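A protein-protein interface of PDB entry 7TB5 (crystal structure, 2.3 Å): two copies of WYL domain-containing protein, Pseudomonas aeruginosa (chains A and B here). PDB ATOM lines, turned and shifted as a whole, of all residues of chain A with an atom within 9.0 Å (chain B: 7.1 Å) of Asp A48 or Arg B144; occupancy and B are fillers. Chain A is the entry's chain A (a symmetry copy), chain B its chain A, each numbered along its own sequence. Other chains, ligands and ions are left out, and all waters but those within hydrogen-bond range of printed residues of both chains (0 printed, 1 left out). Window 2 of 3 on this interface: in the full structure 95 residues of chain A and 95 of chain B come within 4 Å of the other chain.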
ATOM      1  N   PHE A  30     -29.204   4.508 -34.457  1.00  0.00           N
ATOM      2  CA  PHE A  30     -29.206   5.286 -33.215  1.00  0.00           C
ATOM      3  C   PHE A  30     -30.302   6.360 -33.230  1.00  0.00           C
ATOM      4  O   PHE A  30     -31.115   6.460 -32.297  1.00  0.00           O
ATOM      5  CB  PHE A  30     -27.824   5.905 -33.031  1.00  0.00           C
ATOM      6  CG  PHE A  30     -27.639   6.663 -31.749  1.00  0.00           C
ATOM      7  CD1 PHE A  30     -27.259   6.012 -30.600  1.00  0.00           C
ATOM      8  CD2 PHE A  30     -27.810   8.032 -31.706  1.00  0.00           C
ATOM      9  CE1 PHE A  30     -27.072   6.715 -29.419  1.00  0.00           C
ATOM     10  CE2 PHE A  30     -27.598   8.736 -30.552  1.00  0.00           C
ATOM     11  CZ  PHE A  30     -27.225   8.085 -29.402  1.00  0.00           C
ATOM     12  N   ARG A  34     -33.413   6.292 -30.731  1.00  0.00           N
ATOM     13  CA  ARG A  34     -33.673   7.338 -29.735  1.00  0.00           C
ATOM     14  C   ARG A  34     -35.088   7.879 -29.893  1.00  0.00           C
ATOM     15  O   ARG A  34     -35.767   8.183 -28.900  1.00  0.00           O
ATOM     16  CB  ARG A  34     -32.669   8.505 -29.832  1.00  0.00           C
ATOM     17  CG  ARG A  34     -31.213   8.167 -29.604  1.00  0.00           C
ATOM     18  CD  ARG A  34     -30.777   8.232 -28.145  1.00  0.00           C
ATOM     19  NE  ARG A  34     -31.453   9.228 -27.333  1.00  0.00           N
ATOM     20  CZ  ARG A  34     -30.873  10.295 -26.807  1.00  0.00           C
ATOM     21  NH1 ARG A  34     -29.611  10.594 -27.048  1.00  0.00           N
ATOM     22  NH2 ARG A  34     -31.583  11.088 -26.025  1.00  0.00           N
ATOM     23  N   ASN A  42     -30.921  14.918 -29.741  1.00  0.00           N
ATOM     24  CA  ASN A  42     -30.111  16.123 -29.876  1.00  0.00           C
ATOM     25  C   ASN A  42     -28.995  15.869 -30.886  1.00  0.00           C
ATOM     26  O   ASN A  42     -28.447  14.768 -30.961  1.00  0.00           O
ATOM     27  CB  ASN A  42     -29.533  16.473 -28.500  1.00  0.00           C
ATOM     28  CG  ASN A  42     -29.040  17.904 -28.401  1.00  0.00           C
ATOM     29  OD1 ASN A  42     -28.535  18.490 -29.366  1.00  0.00           O
ATOM     30  ND2 ASN A  42     -29.186  18.481 -27.218  1.00  0.00           N
ATOM     31  N   ARG A  43     -28.657  16.886 -31.675  1.00  0.00           N
ATOM     32  CA  ARG A  43     -27.506  16.746 -32.564  1.00  0.00           C
ATOM     33  C   ARG A  43     -26.231  16.426 -31.789  1.00  0.00           C
ATOM     34  O   ARG A  43     -25.386  15.659 -32.263  1.00  0.00           O
ATOM     35  CB  ARG A  43     -27.313  18.017 -33.385  1.00  0.00           C
ATOM     36  CG  ARG A  43     -26.137  17.963 -34.338  1.00  0.00           C
ATOM     37  CD  ARG A  43     -26.201  19.043 -35.413  1.00  0.00           C
ATOM     38  NE  ARG A  43     -26.342  20.363 -34.816  1.00  0.00           N
ATOM     39  CZ  ARG A  43     -26.086  21.501 -35.439  1.00  0.00           C
ATOM     40  NH1 ARG A  43     -25.639  21.524 -36.685  1.00  0.00           N
ATOM     41  NH2 ARG A  43     -26.289  22.647 -34.796  1.00  0.00           N
ATOM     42  N   SER A  44     -26.081  16.980 -30.583  1.00  0.00           N
ATOM     43  CA  SER A  44     -24.894  16.706 -29.777  1.00  0.00           C
ATOM     44  C   SER A  44     -24.897  15.304 -29.187  1.00  0.00           C
ATOM     45  O   SER A  44     -23.852  14.847 -28.711  1.00  0.00           O
ATOM     46  CB  SER A  44     -24.766  17.736 -28.641  1.00  0.00           C
ATOM     47  OG  SER A  44     -25.809  17.588 -27.694  1.00  0.00           O
ATOM     48  N   SER A  45     -26.039  14.614 -29.199  1.00  0.00           N
ATOM     49  CA  SER A  45     -26.032  13.201 -28.844  1.00  0.00           C
ATOM     50  C   SER A  45     -25.229  12.384 -29.851  1.00  0.00           C
ATOM     51  O   SER A  45     -24.472  11.478 -29.476  1.00  0.00           O
ATOM     52  CB  SER A  45     -27.458  12.673 -28.763  1.00  0.00           C
ATOM     53  OG  SER A  45     -27.421  11.335 -28.343  1.00  0.00           O
ATOM     54  N   LEU A  46     -25.382  12.691 -31.137  1.00  0.00           N
ATOM     55  CA  LEU A  46     -24.628  11.971 -32.152  1.00  0.00           C
ATOM     56  C   LEU A  46     -23.141  12.268 -32.024  1.00  0.00           C
ATOM     57  O   LEU A  46     -22.309  11.354 -32.095  1.00  0.00           O
ATOM     58  CB  LEU A  46     -25.133  12.343 -33.542  1.00  0.00           C
ATOM     59  CG  LEU A  46     -26.488  11.840 -34.003  1.00  0.00           C
ATOM     60  CD1 LEU A  46     -26.916  12.630 -35.261  1.00  0.00           C
ATOM     61  CD2 LEU A  46     -26.448  10.310 -34.303  1.00  0.00           C
ATOM     62  N   THR A  47     -22.784  13.547 -31.816  1.00  0.00           N
ATOM     63  CA  THR A  47     -21.368  13.899 -31.719  1.00  0.00           C
ATOM     64  C   THR A  47     -20.756  13.321 -30.448  1.00  0.00           C
ATOM     65  O   THR A  47     -19.607  12.858 -30.448  1.00  0.00           O
ATOM     66  CB  THR A  47     -21.155  15.421 -31.739  1.00  0.00           C
ATOM     67  OG1 THR A  47     -21.885  16.009 -30.663  1.00  0.00           O
ATOM     68  CG2 THR A  47     -21.635  16.043 -33.027  1.00  0.00           C
ATOM     69  N   ASP A  48     -21.495  13.358 -29.343  1.00  0.00           N
ATOM     70  CA  ASP A  48     -20.951  12.803 -28.111  1.00  0.00           C
ATOM     71  C   ASP A  48     -20.720  11.305 -28.252  1.00  0.00           C
ATOM     72  O   ASP A  48     -19.649  10.788 -27.909  1.00  0.00           O
ATOM     73  CB  ASP A  48     -21.894  13.069 -26.941  1.00  0.00           C
ATOM     74  CG  ASP A  48     -21.825  14.471 -26.443  1.00  0.00           C
ATOM     75  OD1 ASP A  48     -21.050  15.311 -27.000  1.00  0.00           O
ATOM     76  OD2 ASP A  48     -22.562  14.725 -25.465  1.00  0.00           O
ATOM     77  N   PHE A  49     -21.727  10.595 -28.763  1.00  0.00           N
ATOM     78  CA  PHE A  49     -21.748   9.138 -28.747  1.00  0.00           C
ATOM     79  C   PHE A  49     -20.775   8.559 -29.765  1.00  0.00           C
ATOM     80  O   PHE A  49     -20.090   7.576 -29.473  1.00  0.00           O
ATOM     81  CB  PHE A  49     -23.187   8.664 -29.011  1.00  0.00           C
ATOM     82  CG  PHE A  49     -23.447   7.230 -28.661  1.00  0.00           C
ATOM     83  CD1 PHE A  49     -23.042   6.219 -29.504  1.00  0.00           C
ATOM     84  CD2 PHE A  49     -24.128   6.897 -27.509  1.00  0.00           C
ATOM     85  CE1 PHE A  49     -23.297   4.898 -29.203  1.00  0.00           C
ATOM     86  CE2 PHE A  49     -24.383   5.575 -27.199  1.00  0.00           C
ATOM     87  CZ  PHE A  49     -23.963   4.576 -28.048  1.00  0.00           C
ATOM     88  N   PHE A  50     -20.695   9.155 -30.958  1.00  0.00           N
ATOM     89  CA  PHE A  50     -19.915   8.596 -32.055  1.00  0.00           C
ATOM     90  C   PHE A  50     -18.632   9.348 -32.347  1.00  0.00           C
ATOM     91  O   PHE A  50     -17.839   8.883 -33.172  1.00  0.00           O
ATOM     92  CB  PHE A  50     -20.760   8.564 -33.335  1.00  0.00           C
ATOM     93  CG  PHE A  50     -21.897   7.591 -33.280  1.00  0.00           C
ATOM     94  CD1 PHE A  50     -21.678   6.254 -33.568  1.00  0.00           C
ATOM     95  CD2 PHE A  50     -23.176   8.007 -32.968  1.00  0.00           C
ATOM     96  CE1 PHE A  50     -22.705   5.358 -33.528  1.00  0.00           C
ATOM     97  CE2 PHE A  50     -24.216   7.098 -32.915  1.00  0.00           C
ATOM     98  CZ  PHE A  50     -23.981   5.791 -33.204  1.00  0.00           C
ATOM     99  N   GLY A  51     -18.424  10.505 -31.732  1.00  0.00           N
ATOM    100  CA  GLY A  51     -17.229  11.282 -31.982  1.00  0.00           C
ATOM    101  C   GLY A  51     -17.151  11.900 -33.357  1.00  0.00           C
ATOM    102  O   GLY A  51     -16.048  12.081 -33.880  1.00  0.00           O
ATOM    103  N   ILE A  52     -18.286  12.226 -33.959  1.00  0.00           N
ATOM    104  CA  ILE A  52     -18.317  12.796 -35.289  1.00  0.00           C
ATOM    105  C   ILE A  52     -18.418  14.309 -35.172  1.00  0.00           C
ATOM    106  O   ILE A  52     -18.720  14.864 -34.112  1.00  0.00           O
ATOM    107  CB  ILE A  52     -19.483  12.230 -36.125  1.00  0.00           C
ATOM    108  CG1 ILE A  52     -20.814  12.453 -35.410  1.00  0.00           C
ATOM    109  CG2 ILE A  52     -19.293  10.720 -36.408  1.00  0.00           C
ATOM    110  CD1 ILE A  52     -22.032  12.062 -36.249  1.00  0.00           C
ATOM    111  N   SER A  53     -18.158  14.988 -36.281  1.00  0.00           N
ATOM    112  CA  SER A  53     -18.230  16.430 -36.298  1.00  0.00           C
ATOM    113  C   SER A  53     -19.683  16.868 -36.298  1.00  0.00           C
ATOM    114  O   SER A  53     -20.592  16.101 -36.635  1.00  0.00           O
ATOM    115  CB  SER A  53     -17.523  16.983 -37.526  1.00  0.00           C
ATOM    116  OG  SER A  53     -18.271  16.701 -38.689  1.00  0.00           O
ATOM    117  N   VAL A  54     -19.899  18.119 -35.891  1.00  0.00           N
ATOM    118  CA  VAL A  54     -21.235  18.697 -35.967  1.00  0.00           C
ATOM    119  C   VAL A  54     -21.758  18.661 -37.396  1.00  0.00           C
ATOM    120  O   VAL A  54     -22.913  18.273 -37.602  1.00  0.00           O
ATOM    121  CB  VAL A  54     -21.245  20.105 -35.365  1.00  0.00           C
ATOM    122  CG1 VAL A  54     -22.498  20.867 -35.786  1.00  0.00           C
ATOM    123  CG2 VAL A  54     -21.172  20.020 -33.857  1.00  0.00           C
ATOM    124  N   ALA A  57     -22.991  15.168 -38.135  1.00  0.00           N
ATOM    125  CA  ALA A  57     -24.250  14.897 -37.455  1.00  0.00           C
ATOM    126  C   ALA A  57     -25.404  15.548 -38.193  1.00  0.00           C
ATOM    127  O   ALA A  57     -26.527  15.042 -38.170  1.00  0.00           O
ATOM    128  CB  ALA A  57     -24.199  15.403 -36.009  1.00  0.00           C
ATOM    129  N   LEU A 104     -23.502   0.537 -28.679  1.00  0.00           N
ATOM    130  CA  LEU A 104     -22.363   0.862 -27.830  1.00  0.00           C
ATOM    131  C   LEU A 104     -21.220  -0.135 -27.992  1.00  0.00           C
ATOM    132  O   LEU A 104     -20.050   0.241 -28.013  1.00  0.00           O
ATOM    133  CB  LEU A 104     -22.850   0.907 -26.383  1.00  0.00           C
ATOM    134  CG  LEU A 104     -21.882   1.367 -25.300  1.00  0.00           C
ATOM    135  CD1 LEU A 104     -21.370   2.736 -25.647  1.00  0.00           C
ATOM    136  CD2 LEU A 104     -22.606   1.377 -23.968  1.00  0.00           C
ATOM    137  N   PRO A 123     -12.098   2.494 -25.637  1.00  0.00           N
ATOM    138  CA  PRO A 123     -13.197   3.206 -24.941  1.00  0.00           C
ATOM    139  C   PRO A 123     -14.123   2.242 -24.181  1.00  0.00           C
ATOM    140  O   PRO A 123     -14.499   2.516 -23.039  1.00  0.00           O
ATOM    141  CB  PRO A 123     -14.008   3.898 -26.065  1.00  0.00           C
ATOM    142  CG  PRO A 123     -13.285   3.598 -27.353  1.00  0.00           C
ATOM    143  CD  PRO A 123     -12.284   2.451 -27.096  1.00  0.00           C
ATOM    144  N   ALA B 136     -29.030   6.906 -22.995  1.00  0.00           N
ATOM    145  CA  ALA B 136     -28.096   7.239 -24.069  1.00  0.00           C
ATOM    146  C   ALA B 136     -27.422   8.603 -23.893  1.00  0.00           C
ATOM    147  O   ALA B 136     -26.275   8.776 -24.319  1.00  0.00           O
ATOM    148  CB  ALA B 136     -28.830   7.188 -25.401  1.00  0.00           C
ATOM    149  N   ASP B 137     -28.099   9.576 -23.277  1.00  0.00           N
ATOM    150  CA  ASP B 137     -27.466  10.864 -23.011  1.00  0.00           C
ATOM    151  C   ASP B 137     -26.266  10.716 -22.081  1.00  0.00           C
ATOM    152  O   ASP B 137     -25.179  11.245 -22.352  1.00  0.00           O
ATOM    153  CB  ASP B 137     -28.484  11.794 -22.378  1.00  0.00           C
ATOM    154  CG  ASP B 137     -29.537  12.285 -23.355  1.00  0.00           C
ATOM    155  OD1 ASP B 137     -29.180  12.594 -24.506  1.00  0.00           O
ATOM    156  OD2 ASP B 137     -30.716  12.392 -22.948  1.00  0.00           O
ATOM    157  N   ILE B 138     -26.461  10.020 -20.954  1.00  0.00           N
ATOM    158  CA  ILE B 138     -25.378   9.815 -19.996  1.00  0.00           C
ATOM    159  C   ILE B 138     -24.254   8.999 -20.618  1.00  0.00           C
ATOM    160  O   ILE B 138     -23.069   9.303 -20.417  1.00  0.00           O
ATOM    161  CB  ILE B 138     -25.933   9.168 -18.712  1.00  0.00           C
ATOM    162  CG1 ILE B 138     -26.766  10.216 -17.954  1.00  0.00           C
ATOM    163  CG2 ILE B 138     -24.814   8.653 -17.816  1.00  0.00           C
ATOM    164  CD1 ILE B 138     -27.756   9.656 -16.974  1.00  0.00           C
ATOM    165  N   VAL B 139     -24.594   7.961 -21.387  1.00  0.00           N
ATOM    166  CA  VAL B 139     -23.556   7.173 -22.048  1.00  0.00           C
ATOM    167  C   VAL B 139     -22.746   8.038 -23.004  1.00  0.00           C
ATOM    168  O   VAL B 139     -21.518   7.943 -23.070  1.00  0.00           O
ATOM    169  CB  VAL B 139     -24.171   5.975 -22.793  1.00  0.00           C
ATOM    170  CG1 VAL B 139     -23.161   5.367 -23.733  1.00  0.00           C
ATOM    171  CG2 VAL B 139     -24.653   4.930 -21.830  1.00  0.00           C
ATOM    172  N   GLY B 140     -23.418   8.865 -23.790  1.00  0.00           N
ATOM    173  CA  GLY B 140     -22.699   9.738 -24.707  1.00  0.00           C
ATOM    174  C   GLY B 140     -21.742  10.711 -24.029  1.00  0.00           C
ATOM    175  O   GLY B 140     -20.618  10.905 -24.497  1.00  0.00           O
ATOM    176  N   VAL B 141     -22.175  11.363 -22.943  1.00  0.00           N
ATOM    177  CA  VAL B 141     -21.266  12.265 -22.234  1.00  0.00           C
ATOM    178  C   VAL B 141     -20.048  11.502 -21.723  1.00  0.00           C
ATOM    179  O   VAL B 141     -18.913  11.991 -21.791  1.00  0.00           O
ATOM    180  CB  VAL B 141     -21.994  12.988 -21.087  1.00  0.00           C
ATOM    181  CG1 VAL B 141     -20.980  13.884 -20.306  1.00  0.00           C
ATOM    182  CG2 VAL B 141     -23.130  13.843 -21.627  1.00  0.00           C
ATOM    183  N   ILE B 142     -20.254  10.277 -21.236  1.00  0.00           N
ATOM    184  CA  ILE B 142     -19.134   9.506 -20.704  1.00  0.00           C
ATOM    185  C   ILE B 142     -18.187   9.091 -21.821  1.00  0.00           C
ATOM    186  O   ILE B 142     -16.961   9.106 -21.652  1.00  0.00           O
ATOM    187  CB  ILE B 142     -19.645   8.282 -19.925  1.00  0.00           C
ATOM    188  CG1 ILE B 142     -20.313   8.731 -18.627  1.00  0.00           C
ATOM    189  CG2 ILE B 142     -18.515   7.311 -19.682  1.00  0.00           C
ATOM    190  CD1 ILE B 142     -20.999   7.626 -17.853  1.00  0.00           C
ATOM    191  N   LEU B 143     -18.732   8.682 -22.970  1.00  0.00           N
ATOM    192  CA  LEU B 143     -17.879   8.343 -24.108  1.00  0.00           C
ATOM    193  C   LEU B 143     -17.069   9.559 -24.549  1.00  0.00           C
ATOM    194  O   LEU B 143     -15.854   9.474 -24.767  1.00  0.00           O
ATOM    195  CB  LEU B 143     -18.730   7.793 -25.267  1.00  0.00           C
ATOM    196  CG  LEU B 143     -19.278   6.386 -25.073  1.00  0.00           C
ATOM    197  CD1 LEU B 143     -20.234   6.003 -26.174  1.00  0.00           C
ATOM    198  CD2 LEU B 143     -18.119   5.372 -25.011  1.00  0.00           C
ATOM    199  N   ARG B 144     -17.718  10.709 -24.685  1.00  0.00           N
ATOM    200  CA  ARG B 144     -16.970  11.931 -24.982  1.00  0.00           C
ATOM    201  C   ARG B 144     -15.836  12.167 -23.982  1.00  0.00           C
ATOM    202  O   ARG B 144     -14.690  12.447 -24.360  1.00  0.00           O
ATOM    203  CB  ARG B 144     -17.904  13.133 -24.961  1.00  0.00           C
ATOM    204  CG  ARG B 144     -17.184  14.447 -25.297  1.00  0.00           C
ATOM    205  CD  ARG B 144     -18.078  15.656 -25.066  1.00  0.00           C
ATOM    206  NE  ARG B 144     -17.373  16.885 -25.411  1.00  0.00           N
ATOM    207  CZ  ARG B 144     -17.799  18.099 -25.097  1.00  0.00           C
ATOM    208  NH1 ARG B 144     -18.913  18.283 -24.412  1.00  0.00           N
ATOM    209  NH2 ARG B 144     -17.093  19.155 -25.487  1.00  0.00           N
ATOM    210  N   ALA B 145     -16.148  12.084 -22.694  1.00  0.00           N
ATOM    211  CA  ALA B 145     -15.126  12.332 -21.686  1.00  0.00           C
ATOM    212  C   ALA B 145     -13.995  11.316 -21.769  1.00  0.00           C
ATOM    213  O   ALA B 145     -12.840  11.648 -21.500  1.00  0.00           O
ATOM    214  CB  ALA B 145     -15.756  12.314 -20.295  1.00  0.00           C
ATOM    215  N   ILE B 146     -14.294  10.061 -22.083  1.00  0.00           N
ATOM    216  CA  ILE B 146     -13.217   9.088 -22.240  1.00  0.00           C
ATOM    217  C   ILE B 146     -12.362   9.444 -23.450  1.00  0.00           C
ATOM    218  O   ILE B 146     -11.128   9.482 -23.375  1.00  0.00           O
ATOM    219  CB  ILE B 146     -13.788   7.668 -22.377  1.00  0.00           C
ATOM    220  CG1 ILE B 146     -14.471   7.216 -21.094  1.00  0.00           C
ATOM    221  CG2 ILE B 146     -12.698   6.680 -22.715  1.00  0.00           C
ATOM    222  CD1 ILE B 146     -15.402   6.023 -21.285  1.00  0.00           C
ATOM    223  N   ARG B 147     -13.009   9.708 -24.587  1.00  0.00           N
ATOM    224  CA  ARG B 147     -12.292  10.054 -25.813  1.00  0.00           C
ATOM    225  C   ARG B 147     -11.388  11.267 -25.623  1.00  0.00           C
ATOM    226  O   ARG B 147     -10.246  11.283 -26.099  1.00  0.00           O
ATOM    227  CB  ARG B 147     -13.308  10.330 -26.913  1.00  0.00           C
ATOM    228  CG  ARG B 147     -12.912   9.923 -28.290  1.00  0.00           C
ATOM    229  CD  ARG B 147     -14.190   9.643 -29.079  1.00  0.00           C
ATOM    230  NE  ARG B 147     -15.134  10.737 -28.885  1.00  0.00           N
ATOM    231  CZ  ARG B 147     -16.446  10.584 -28.808  1.00  0.00           C
ATOM    232  NH1 ARG B 147     -17.006   9.388 -28.890  1.00  0.00           N
ATOM    233  NH2 ARG B 147     -17.217  11.657 -28.647  1.00  0.00           N
ATOM    234  N   GLU B 148     -11.898  12.310 -24.964  1.00  0.00           N
ATOM    235  CA  GLU B 148     -11.189  13.577 -24.808  1.00  0.00           C
ATOM    236  C   GLU B 148     -10.485  13.722 -23.464  1.00  0.00           C
ATOM    237  O   GLU B 148      -9.977  14.808 -23.153  1.00  0.00           O
ATOM    238  CB  GLU B 148     -12.159  14.745 -24.985  1.00  0.00           C
ATOM    239  CG  GLU B 148     -12.937  14.706 -26.294  1.00  0.00           C
ATOM    240  CD  GLU B 148     -13.905  15.866 -26.417  1.00  0.00           C
ATOM    241  OE1 GLU B 148     -14.090  16.590 -25.407  1.00  0.00           O
ATOM    242  OE2 GLU B 148     -14.498  16.043 -27.507  1.00  0.00           O
ATOM    243  N   THR B 149     -10.442  12.664 -22.663  1.00  0.00           N
ATOM    244  CA  THR B 149      -9.814  12.711 -21.348  1.00  0.00           C
ATOM    245  C   THR B 149     -10.375  13.872 -20.535  1.00  0.00           C
ATOM    246  O   THR B 149      -9.647  14.688 -19.975  1.00  0.00           O
ATOM    247  CB  THR B 149      -8.299  12.828 -21.460  1.00  0.00           C
ATOM    248  OG1 THR B 149      -7.825  11.908 -22.445  1.00  0.00           O
ATOM    249  CG2 THR B 149      -7.648  12.507 -20.122  1.00  0.00           C
ATOM    250  N   GLY B 150     -11.684  13.922 -20.457  1.00  0.00           N
ATOM    251  CA  GLY B 150     -12.374  15.031 -19.841  1.00  0.00           C
ATOM    252  C   GLY B 150     -12.756  14.809 -18.389  1.00  0.00           C
ATOM    253  O   GLY B 150     -12.800  13.680 -17.897  1.00  0.00           O
ATOM    254  N   ILE B 152     -15.808  14.997 -15.767  1.00  0.00           N
ATOM    255  CA  ILE B 152     -17.267  14.994 -15.737  1.00  0.00           C
ATOM    256  C   ILE B 152     -17.765  15.151 -14.308  1.00  0.00           C
ATOM    257  O   ILE B 152     -17.137  14.690 -13.353  1.00  0.00           O
ATOM    258  CB  ILE B 152     -17.920  13.729 -16.349  1.00  0.00           C
ATOM    259  CG1 ILE B 152     -17.394  12.451 -15.709  1.00  0.00           C
ATOM    260  CG2 ILE B 152     -17.730  13.674 -17.834  1.00  0.00           C
ATOM    261  CD1 ILE B 152     -18.076  11.204 -16.232  1.00  0.00           C
ATOM    262  N   PRO B 171     -13.110   9.678 -16.260  1.00  0.00           N
ATOM    263  CA  PRO B 171     -13.202   8.290 -16.686  1.00  0.00           C
ATOM    264  C   PRO B 171     -12.257   7.941 -17.816  1.00  0.00           C
ATOM    265  O   PRO B 171     -11.902   8.787 -18.662  1.00  0.00           O
ATOM    266  CB  PRO B 171     -14.641   8.206 -17.185  1.00  0.00           C
ATOM    267  CG  PRO B 171     -14.886   9.538 -17.809  1.00  0.00           C
ATOM    268  CD  PRO B 171     -14.134  10.510 -16.891  1.00  0.00           C
ATOM    269  N   TYR B 206     -20.329  17.048 -18.883  1.00  0.00           N
ATOM    270  CA  TYR B 206     -18.933  17.309 -19.226  1.00  0.00           C
ATOM    271  C   TYR B 206     -18.573  18.745 -18.867  1.00  0.00           C
ATOM    272  O   TYR B 206     -19.250  19.693 -19.286  1.00  0.00           O
ATOM    273  CB  TYR B 206     -18.720  17.067 -20.716  1.00  0.00           C
ATOM    274  CG  TYR B 206     -17.319  17.251 -21.239  1.00  0.00           C
ATOM    275  CD1 TYR B 206     -16.849  18.509 -21.583  1.00  0.00           C
ATOM    276  CD2 TYR B 206     -16.482  16.170 -21.423  1.00  0.00           C
ATOM    277  CE1 TYR B 206     -15.577  18.690 -22.066  1.00  0.00           C
ATOM    278  CE2 TYR B 206     -15.200  16.339 -21.919  1.00  0.00           C
ATOM    279  CZ  TYR B 206     -14.753  17.605 -22.235  1.00  0.00           C
ATOM    280  OH  TYR B 206     -13.476  17.800 -22.726  1.00  0.00           O
ATOM    281  N   VAL B 207     -17.511  18.922 -18.083  1.00  0.00           N
ATOM    282  CA  VAL B 207     -17.216  20.240 -17.546  1.00  0.00           C
ATOM    283  C   VAL B 207     -15.800  20.730 -17.833  1.00  0.00           C
ATOM    284  O   VAL B 207     -15.527  21.934 -17.711  1.00  0.00           O
ATOM    285  CB  VAL B 207     -17.479  20.246 -16.029  1.00  0.00           C
ATOM    286  CG1 VAL B 207     -18.950  20.136 -15.729  1.00  0.00           C
ATOM    287  CG2 VAL B 207     -16.758  19.091 -15.359  1.00  0.00           C
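No position is printed for both chains.
CD of Arg A34 touches CB of Ala B136, at 3.5 Å.
Asp A48 touches Gly B140 (CB to O, 3.5 Å).
Asp A48 touches Val B141 (OD2 to CG2, 3.98 Å).
OD1 of Asp A48 touches CD of Arg B144, at 3.6 Å.
Phe A49 touches Val B139.
O of Phe A49 touches CD1 of Leu B143, at 3.7 Å.
O of Phe A49 touches NH1 of Arg B147, 3.6 Å away.
Arg B147 touches Phe A50.
Leu A104 touches Val B139 (CD1 to CG1, 3.7 Å).
Leu A104 touches Leu B143 (CD1 to CD1, 3.5 Å).
Printed residues of chain A that touch a printed residue of chain B: Arg A34, Thr A47, Asp A48, Phe A49, Phe A50, Gly A51 and Leu A104.
Printed residues of chain B that touch a printed residue of chain A: Ala B136, Asp B137, Val B139, Gly B140, Val B141, Leu B143, Arg B144 and Arg B147.
Hydrophobic or aromatic side chains of chain B within 4 Å of the printed part of chain A: Ala B136, Val B139, Val B141 and Leu B143.
Among the printed residues, 14 pairs touch across the chains.
Among the printed residues, Asp or Glu carboxylates within 4 Å of a Lys or Arg side-chain nitrogen of the other chain: Arg A34 with Asp B137.
NH2 of Arg B147 sits at hydrogen-bond distance from O of Asp A48 (2.7 Å).
NH2 of Arg B147 is in hydrogen-bond range of O of Thr A47 (3.2 Å).
The side-chain carboxylate (OD1) of Asp B137 is in salt-bridge range of the guanidinium group (NH2) of Arg A34, 3.2 Å away.
NH1 of Arg B147 sits close to N of Gly A51 (3.4 Å).
Of the printed residues of chain B, Asp A48 touches Gly B140 (3.5 Å), Val B141 (3.98 Å), Arg B144 (3.6 Å) and Arg B147 (2.7 Å).
Ala B145 touches none of the printed residues of chain A.
Of the printed residues of chain A, Leu B143 touches Phe A49 and Leu A104.
Of the printed residues of chain B, Arg A34 touches Ala B136 and Asp B137.
Printed residues of chain A within 4 Å of Arg B147: Thr A47, Asp A48, Phe A49, Phe A50 and Gly A51.
Printed residues of chain B within 4 Å of Leu A104: Val B139 (3.7 Å) and Leu B143 (3.5 Å).
Ala A57 touches none of the printed residues of chain B.
The nearest printed residue of chain B that does not touch Thr A47 is Arg B144 (5.8 Å).
The side-chain hydroxyl of Ser A45 sits at hydrogen-bond distance from the guanidinium group of Arg A34 (2.6 Å).
The guanidinium group (NE) of Arg B144 lies within salt-bridge range of the side-chain carboxylate (OE1) of Glu B148 (3.3 Å).
OG1 of Thr A47 sits at hydrogen-bond distance from O of Ser A44, at 3.0 Å.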
